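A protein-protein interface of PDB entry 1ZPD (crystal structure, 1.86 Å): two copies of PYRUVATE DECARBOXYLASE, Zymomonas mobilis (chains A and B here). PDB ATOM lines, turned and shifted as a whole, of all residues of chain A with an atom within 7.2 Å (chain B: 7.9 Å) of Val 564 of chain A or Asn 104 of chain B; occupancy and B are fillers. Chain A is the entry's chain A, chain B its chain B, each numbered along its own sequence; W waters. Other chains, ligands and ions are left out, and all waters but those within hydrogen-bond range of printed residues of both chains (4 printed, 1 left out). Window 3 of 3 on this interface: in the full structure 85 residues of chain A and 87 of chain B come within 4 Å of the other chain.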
ATOM      1  N   ALA A 558     -26.337 -22.944  -4.885  1.00  0.00           N
ATOM      2  CA  ALA A 558     -24.988 -23.498  -4.707  1.00  0.00           C
ATOM      3  C   ALA A 558     -24.397 -23.934  -6.061  1.00  0.00           C
ATOM      4  O   ALA A 558     -23.216 -23.656  -6.344  1.00  0.00           O
ATOM      5  CB  ALA A 558     -25.013 -24.662  -3.725  1.00  0.00           C
ATOM      6  N   SER A 560     -24.971 -22.842  -9.094  1.00  0.00           N
ATOM      7  CA  SER A 560     -24.649 -21.782 -10.063  1.00  0.00           C
ATOM      8  C   SER A 560     -23.762 -20.697  -9.499  1.00  0.00           C
ATOM      9  O   SER A 560     -23.473 -19.772 -10.273  1.00  0.00           O
ATOM     10  CB  SER A 560     -25.968 -21.200 -10.611  1.00  0.00           C
ATOM     11  OG  SER A 560     -26.628 -20.514  -9.538  1.00  0.00           O
ATOM     12  N   ARG A 561     -23.288 -20.772  -8.245  1.00  0.00           N
ATOM     13  CA  ARG A 561     -22.491 -19.671  -7.709  1.00  0.00           C
ATOM     14  C   ARG A 561     -21.249 -19.417  -8.583  1.00  0.00           C
ATOM     15  O   ARG A 561     -20.553 -20.308  -9.065  1.00  0.00           O
ATOM     16  CB  ARG A 561     -22.088 -19.913  -6.250  1.00  0.00           C
ATOM     17  CG  ARG A 561     -21.075 -21.033  -6.017  1.00  0.00           C
ATOM     18  CD  ARG A 561     -20.958 -21.276  -4.503  1.00  0.00           C
ATOM     19  NE  ARG A 561     -19.843 -22.154  -4.132  1.00  0.00           N
ATOM     20  CZ  ARG A 561     -19.817 -23.476  -4.272  1.00  0.00           C
ATOM     21  NH1 ARG A 561     -20.857 -24.100  -4.814  1.00  0.00           N
ATOM     22  NH2 ARG A 561     -18.740 -24.170  -3.874  1.00  0.00           N
ATOM     23  N   LYS A 562     -20.940 -18.138  -8.759  1.00  0.00           N
ATOM     24  CA  LYS A 562     -19.894 -17.725  -9.715  1.00  0.00           C
ATOM     25  C   LYS A 562     -18.487 -18.166  -9.307  1.00  0.00           C
ATOM     26  O   LYS A 562     -18.172 -18.316  -8.119  1.00  0.00           O
ATOM     27  CB  LYS A 562     -19.889 -16.190  -9.826  1.00  0.00           C
ATOM     28  CG  LYS A 562     -21.085 -15.666 -10.630  1.00  0.00           C
ATOM     29  CD  LYS A 562     -21.288 -14.180 -10.379  1.00  0.00           C
ATOM     30  CE  LYS A 562     -22.535 -13.662 -11.098  1.00  0.00           C
ATOM     31  NZ  LYS A 562     -22.582 -14.110 -12.531  1.00  0.00           N
ATOM     32  N   PRO A 563     -17.620 -18.368 -10.306  1.00  0.00           N
ATOM     33  CA  PRO A 563     -16.217 -18.671 -10.066  1.00  0.00           C
ATOM     34  C   PRO A 563     -15.606 -17.580  -9.193  1.00  0.00           C
ATOM     35  O   PRO A 563     -15.989 -16.413  -9.345  1.00  0.00           O
ATOM     36  CB  PRO A 563     -15.585 -18.668 -11.474  1.00  0.00           C
ATOM     37  CG  PRO A 563     -16.720 -18.988 -12.393  1.00  0.00           C
ATOM     38  CD  PRO A 563     -17.950 -18.359 -11.768  1.00  0.00           C
ATOM     39  N   VAL A 564     -14.673 -17.936  -8.318  1.00  0.00           N
ATOM     40  CA  VAL A 564     -13.993 -16.967  -7.461  1.00  0.00           C
ATOM     41  C   VAL A 564     -12.623 -16.648  -8.076  1.00  0.00           C
ATOM     42  O   VAL A 564     -12.131 -17.425  -8.907  1.00  0.00           O
ATOM     43  CB  VAL A 564     -13.839 -17.497  -6.016  1.00  0.00           C
ATOM     44  CG1 VAL A 564     -13.127 -16.515  -5.097  1.00  0.00           C
ATOM     45  CG2 VAL A 564     -15.209 -17.832  -5.405  1.00  0.00           C
ATOM     46  N   ASN A 565     -12.001 -15.542  -7.693  1.00  0.00           N
ATOM     47  CA  ASN A 565     -10.728 -15.128  -8.298  1.00  0.00           C
ATOM     48  C   ASN A 565      -9.551 -15.970  -7.810  1.00  0.00           C
ATOM     49  O   ASN A 565      -9.311 -16.102  -6.601  1.00  0.00           O
ATOM     50  CB  ASN A 565     -10.480 -13.643  -8.027  1.00  0.00           C
ATOM     51  CG  ASN A 565      -9.630 -13.011  -9.126  1.00  0.00           C
ATOM     52  OD1 ASN A 565      -8.514 -13.478  -9.410  1.00  0.00           O
ATOM     53  ND2 ASN A 565     -10.146 -11.958  -9.754  1.00  0.00           N
ATOM     54  N   LYS A 566      -8.797 -16.540  -8.756  1.00  0.00           N
ATOM     55  CA  LYS A 566      -7.662 -17.411  -8.465  1.00  0.00           C
ATOM     56  C   LYS A 566      -6.294 -16.742  -8.647  1.00  0.00           C
ATOM     57  O   LYS A 566      -5.282 -17.464  -8.780  1.00  0.00           O
ATOM     58  CB  LYS A 566      -7.718 -18.635  -9.396  1.00  0.00           C
ATOM     59  CG  LYS A 566      -8.979 -19.476  -9.247  1.00  0.00           C
ATOM     60  CD  LYS A 566      -8.862 -20.365  -8.011  1.00  0.00           C
ATOM     61  CE  LYS A 566     -10.053 -21.291  -7.863  1.00  0.00           C
ATOM     62  NZ  LYS A 566      -9.794 -22.617  -8.480  1.00  0.00           N
ATOM     63  N   PRO B 101     -19.058 -30.599 -11.683  1.00  0.00           N
ATOM     64  CA  PRO B 101     -19.142 -29.739 -10.513  1.00  0.00           C
ATOM     65  C   PRO B 101     -18.817 -28.275 -10.767  1.00  0.00           C
ATOM     66  O   PRO B 101     -18.064 -27.883 -11.671  1.00  0.00           O
ATOM     67  CB  PRO B 101     -18.104 -30.342  -9.542  1.00  0.00           C
ATOM     68  CG  PRO B 101     -18.112 -31.788  -9.870  1.00  0.00           C
ATOM     69  CD  PRO B 101     -18.317 -31.854 -11.386  1.00  0.00           C
ATOM     70  N   ASN B 102     -19.434 -27.435  -9.935  1.00  0.00           N
ATOM     71  CA  ASN B 102     -19.086 -26.028  -9.840  1.00  0.00           C
ATOM     72  C   ASN B 102     -17.566 -25.945  -9.738  1.00  0.00           C
ATOM     73  O   ASN B 102     -16.952 -26.702  -8.958  1.00  0.00           O
ATOM     74  CB  ASN B 102     -19.758 -25.447  -8.591  1.00  0.00           C
ATOM     75  CG  ASN B 102     -19.569 -23.957  -8.448  1.00  0.00           C
ATOM     76  OD1 ASN B 102     -18.475 -23.524  -8.077  1.00  0.00           O
ATOM     77  ND2 ASN B 102     -20.642 -23.195  -8.684  1.00  0.00           N
ATOM     78  N   ASN B 103     -16.963 -24.971 -10.436  1.00  0.00           N
ATOM     79  CA  ASN B 103     -15.480 -24.952 -10.511  1.00  0.00           C
ATOM     80  C   ASN B 103     -14.831 -24.570  -9.189  1.00  0.00           C
ATOM     81  O   ASN B 103     -13.628 -24.829  -8.995  1.00  0.00           O
ATOM     82  CB  ASN B 103     -14.994 -24.140 -11.718  1.00  0.00           C
ATOM     83  CG  ASN B 103     -15.166 -22.652 -11.646  1.00  0.00           C
ATOM     84  OD1 ASN B 103     -15.689 -22.087 -10.677  1.00  0.00           O
ATOM     85  ND2 ASN B 103     -14.700 -21.962 -12.707  1.00  0.00           N
ATOM     86  N   ASN B 104     -15.571 -24.030  -8.219  1.00  0.00           N
ATOM     87  CA  ASN B 104     -15.071 -23.695  -6.889  1.00  0.00           C
ATOM     88  C   ASN B 104     -14.891 -24.929  -6.001  1.00  0.00           C
ATOM     89  O   ASN B 104     -14.216 -24.841  -4.965  1.00  0.00           O
ATOM     90  CB  ASN B 104     -16.078 -22.775  -6.156  1.00  0.00           C
ATOM     91  CG  ASN B 104     -16.114 -21.382  -6.746  1.00  0.00           C
ATOM     92  OD1 ASN B 104     -15.100 -20.674  -6.749  1.00  0.00           O
ATOM     93  ND2 ASN B 104     -17.262 -20.984  -7.285  1.00  0.00           N
ATOM     94  N   ASP B 105     -15.445 -26.066  -6.393  1.00  0.00           N
ATOM     95  CA  ASP B 105     -15.370 -27.266  -5.556  1.00  0.00           C
ATOM     96  C   ASP B 105     -14.089 -28.074  -5.769  1.00  0.00           C
ATOM     97  O   ASP B 105     -13.930 -29.101  -5.087  1.00  0.00           O
ATOM     98  CB  ASP B 105     -16.628 -28.110  -5.804  1.00  0.00           C
ATOM     99  CG  ASP B 105     -17.882 -27.439  -5.240  1.00  0.00           C
ATOM    100  OD1 ASP B 105     -17.803 -26.792  -4.175  1.00  0.00           O
ATOM    101  OD2 ASP B 105     -18.958 -27.517  -5.865  1.00  0.00           O
ATOM    102  N   HIS B 106     -13.183 -27.699  -6.690  1.00  0.00           N
ATOM    103  CA  HIS B 106     -11.921 -28.431  -6.828  1.00  0.00           C
ATOM    104  C   HIS B 106     -10.921 -27.902  -5.807  1.00  0.00           C
ATOM    105  O   HIS B 106     -10.913 -26.699  -5.514  1.00  0.00           O
ATOM    106  CB  HIS B 106     -11.356 -28.312  -8.269  1.00  0.00           C
ATOM    107  CG  HIS B 106     -12.320 -28.840  -9.296  1.00  0.00           C
ATOM    108  ND1 HIS B 106     -12.353 -30.162  -9.667  1.00  0.00           N
ATOM    109  CD2 HIS B 106     -13.292 -28.227 -10.027  1.00  0.00           C
ATOM    110  CE1 HIS B 106     -13.294 -30.342 -10.589  1.00  0.00           C
ATOM    111  NE2 HIS B 106     -13.886 -29.181 -10.813  1.00  0.00           N
ATOM    112  N   ALA B 107     -10.136 -28.792  -5.209  1.00  0.00           N
ATOM    113  CA  ALA B 107      -9.158 -28.404  -4.186  1.00  0.00           C
ATOM    114  C   ALA B 107      -9.770 -27.604  -3.038  1.00  0.00           C
ATOM    115  O   ALA B 107      -9.182 -26.648  -2.528  1.00  0.00           O
ATOM    116  CB  ALA B 107      -8.004 -27.645  -4.864  1.00  0.00           C
ATOM    117  N   ALA B 108     -10.937 -28.022  -2.527  1.00  0.00           N
ATOM    118  CA  ALA B 108     -11.692 -27.262  -1.532  1.00  0.00           C
ATOM    119  C   ALA B 108     -12.161 -28.141  -0.354  1.00  0.00           C
ATOM    120  O   ALA B 108     -12.831 -27.650   0.576  1.00  0.00           O
ATOM    121  CB  ALA B 108     -12.923 -26.653  -2.220  1.00  0.00           C
ATOM    122  N   GLY B 109     -11.852 -29.418  -0.428  1.00  0.00           N
ATOM    123  CA  GLY B 109     -12.266 -30.397   0.590  1.00  0.00           C
ATOM    124  C   GLY B 109     -13.789 -30.547   0.593  1.00  0.00           C
ATOM    125  O   GLY B 109     -14.416 -30.764   1.656  1.00  0.00           O
ATOM    126  N   HIS B 110     -14.407 -30.484  -0.598  1.00  0.00           N
ATOM    127  CA  HIS B 110     -15.874 -30.529  -0.670  1.00  0.00           C
ATOM    128  C   HIS B 110     -16.353 -31.862  -1.210  1.00  0.00           C
ATOM    129  O   HIS B 110     -15.926 -32.302  -2.288  1.00  0.00           O
ATOM    130  CB  HIS B 110     -16.449 -29.403  -1.532  1.00  0.00           C
ATOM    131  CG  HIS B 110     -16.335 -28.027  -0.981  1.00  0.00           C
ATOM    132  ND1 HIS B 110     -16.712 -26.924  -1.731  1.00  0.00           N
ATOM    133  CD2 HIS B 110     -15.890 -27.548   0.217  1.00  0.00           C
ATOM    134  CE1 HIS B 110     -16.505 -25.830  -1.019  1.00  0.00           C
ATOM    135  NE2 HIS B 110     -16.012 -26.181   0.163  1.00  0.00           N
ATOM    136  N   LEU B 112     -19.364 -33.877  -2.858  1.00  0.00           N
ATOM    137  CA  LEU B 112     -20.533 -33.511  -3.653  1.00  0.00           C
ATOM    138  C   LEU B 112     -21.463 -34.672  -3.956  1.00  0.00           C
ATOM    139  O   LEU B 112     -20.995 -35.771  -4.219  1.00  0.00           O
ATOM    140  CB  LEU B 112     -20.074 -32.916  -5.016  1.00  0.00           C
ATOM    141  CG  LEU B 112     -19.210 -31.654  -4.915  1.00  0.00           C
ATOM    142  CD1 LEU B 112     -18.727 -31.254  -6.326  1.00  0.00           C
ATOM    143  CD2 LEU B 112     -19.989 -30.509  -4.269  1.00  0.00           C
ATOM    144  N   TYR B 139     -12.822 -26.351 -17.101  1.00  0.00           N
ATOM    145  CA  TYR B 139     -13.025 -25.736 -15.796  1.00  0.00           C
ATOM    146  C   TYR B 139     -13.190 -24.231 -15.844  1.00  0.00           C
ATOM    147  O   TYR B 139     -13.746 -23.635 -14.906  1.00  0.00           O
ATOM    148  CB  TYR B 139     -11.851 -26.108 -14.852  1.00  0.00           C
ATOM    149  CG  TYR B 139     -11.760 -27.595 -14.571  1.00  0.00           C
ATOM    150  CD1 TYR B 139     -12.903 -28.318 -14.197  1.00  0.00           C
ATOM    151  CD2 TYR B 139     -10.558 -28.289 -14.702  1.00  0.00           C
ATOM    152  CE1 TYR B 139     -12.833 -29.674 -13.964  1.00  0.00           C
ATOM    153  CE2 TYR B 139     -10.475 -29.645 -14.452  1.00  0.00           C
ATOM    154  CZ  TYR B 139     -11.620 -30.329 -14.065  1.00  0.00           C
ATOM    155  OH  TYR B 139     -11.561 -31.684 -13.822  1.00  0.00           O
ATOM    156  N   ALA B 167     -17.851 -27.554 -16.309  1.00  0.00           N
ATOM    157  CA  ALA B 167     -18.267 -27.094 -14.961  1.00  0.00           C
ATOM    158  C   ALA B 167     -19.655 -26.459 -15.043  1.00  0.00           C
ATOM    159  O   ALA B 167     -19.876 -25.571 -15.884  1.00  0.00           O
ATOM    160  CB  ALA B 167     -17.233 -26.150 -14.373  1.00  0.00           C
ATOM    161  N   ASN B 169     -21.241 -24.094 -13.458  1.00  0.00           N
ATOM    162  CA  ASN B 169     -21.338 -22.656 -13.305  1.00  0.00           C
ATOM    163  C   ASN B 169     -20.634 -21.865 -14.416  1.00  0.00           C
ATOM    164  O   ASN B 169     -20.514 -20.644 -14.273  1.00  0.00           O
ATOM    165  CB  ASN B 169     -20.808 -22.242 -11.912  1.00  0.00           C
ATOM    166  CG  ASN B 169     -19.335 -22.559 -11.711  1.00  0.00           C
ATOM    167  OD1 ASN B 169     -18.808 -23.520 -12.287  1.00  0.00           O
ATOM    168  ND2 ASN B 169     -18.640 -21.761 -10.915  1.00  0.00           N
ATOM    169  N   ILE B 170     -20.128 -22.489 -15.495  1.00  0.00           N
ATOM    170  CA  ILE B 170     -19.472 -21.704 -16.560  1.00  0.00           C
ATOM    171  C   ILE B 170     -20.202 -21.817 -17.899  1.00  0.00           C
ATOM    172  O   ILE B 170     -19.793 -21.219 -18.914  1.00  0.00           O
ATOM    173  CB  ILE B 170     -17.983 -22.074 -16.773  1.00  0.00           C
ATOM    174  CG1 ILE B 170     -17.822 -23.434 -17.433  1.00  0.00           C
ATOM    175  CG2 ILE B 170     -17.203 -21.962 -15.460  1.00  0.00           C
ATOM    176  CD1 ILE B 170     -16.377 -23.819 -17.785  1.00  0.00           C
HETATM  177  O   HOH W   1     -21.275 -26.909  -4.622  1.00  0.00           O
HETATM  178  O   HOH W   2     -21.509 -18.882 -12.695  1.00  0.00           O
HETATM  179  O   HOH W   3     -13.295 -20.817  -9.484  1.00  0.00           O
HETATM  180  O   HOH W   4     -17.687 -20.139  -3.945  1.00  0.00           O
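O of Arg 561 of chain A lies within hydrogen-bond range of ND2 of Asn 102 of chain B, at 2.9 Å. The guanidinium group of Arg 561 of chain A lies within salt-bridge range of the side-chain carboxylate of Asp 105 of chain B. ND2 of Asn 169 of chain B is in hydrogen-bond range of O of Arg 561 of chain A, 3.0 Å away. The backbone carbonyl oxygen of Lys 562 of chain A lies within hydrogen-bond range of the side-chain amide nitrogen of Asn 104 of chain B (2.9 Å). The backbone NH (N) of Val 564 of chain A sits close to the side-chain amide oxygen (OD1) of Asn 104 of chain B (3.2 Å).
The backbone carbonyl oxygen (O) of Ala 558 of chain A is in hydrogen-bond range of the guanidinium group (NH1) of Arg 561 of chain A, at 2.8 Å. OD1 of Asn 102 of chain B lies within hydrogen-bond range of ND2 of Asn 104 of chain B (2.9 Å). The side-chain amide nitrogen (ND2) of Asn 102 of chain B sits close to the side-chain amide nitrogen (ND2) of Asn 169 of chain B (3.3 Å). O of Tyr 139 of chain B is in hydrogen-bond range of ND2 of Asn 103 of chain B, 2.9 Å away. The side-chain amide oxygen (OD1) of Asn 103 of chain B is in hydrogen-bond range of the side-chain amide nitrogen (ND2) of Asn 169 of chain B (3.0 Å). OD1 of Asp 105 of chain B is in hydrogen-bond range of ND1 of His 110 of chain B.
O of Ala 558 of chain A touches ND2 of Asn 102 of chain B (3.5 Å). Asn 169 of chain B touches Ser 560 of chain A. Arg 561 of chain A touches Asn 104 of chain B (NH2 to CB, 3.8 Å). CE1 of His 110 of chain B touches NH2 of Arg 561 of chain A, 3.99 Å away. Asn 169 of chain B touches Lys 562 of chain A. Asn 103 of chain B touches Pro 563 of chain A (OD1 to CA, 3.5 Å). CA of Pro 563 of chain A touches ND2 of Asn 104 of chain B, 3.8 Å away. ND2 of Asn 169 of chain B touches CD of Pro 563 of chain A (3.6 Å).
Printed residues of chain B within 4 Å of Ser 560 of chain A: Asn 169. Of the printed residues of chain B, Lys 562 of chain A touches Asn 104 (2.9 Å) and Asn 169 (3.9 Å). Of the printed residues of chain B, Val 564 of chain A touches Asn 104. Printed residues of chain A within 4 Å of Asn 102 of chain B: Ala 558 and Arg 561. Asn 104 of chain B touches four residues of chain A. Leu 112 of chain B touches none of the printed residues of chain A.
Hydrophobic or aromatic side chains of chain A within 4 Å of the printed part of chain B: Pro 563 and Val 564. Along chain A the printed residues that touch a printed residue of chain B span positions 558 to 564. Printed residues of chain B that touch a printed residue of chain A: Asn 102, Asn 103, Asn 104, Asp 105, His 110 and Asn 169. Among the printed residues, Asp or Glu carboxylates within 4 Å of a Lys or Arg side-chain nitrogen of the other chain: Arg 561 of chain A with Asp 105 of chain B (2.8 Å).
No position is printed for both chains. Of the 13 pairs that touch across the chains among the printed residues, none has its exchanged pair printed and touching as well.
Water W2 lies within hydrogen-bond range of the backbone carbonyl oxygen (O) of Asn 169 of chain B and the backbone carbonyl oxygen (O) of Ser 560 of chain A. Water W1 bridges the side-chain carboxylate of Asp 105 of chain B and the guanidinium group of Arg 561 of chain A. Water W4 lies within hydrogen-bond range of the guanidinium group of Arg 561 of chain A (3.0 Å) and the side-chain amide nitrogen of Asn 104 of chain B (3.5 Å). Water W3 lies within hydrogen-bond range of the side-chain amide oxygen (OD1) of Asn 103 of chain B (3.0 Å), the side-chain amide oxygen (OD1) of Asn 104 of chain B (3.3 Å) and the backbone NH (N) of Val 564 of chain A (3.4 Å).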
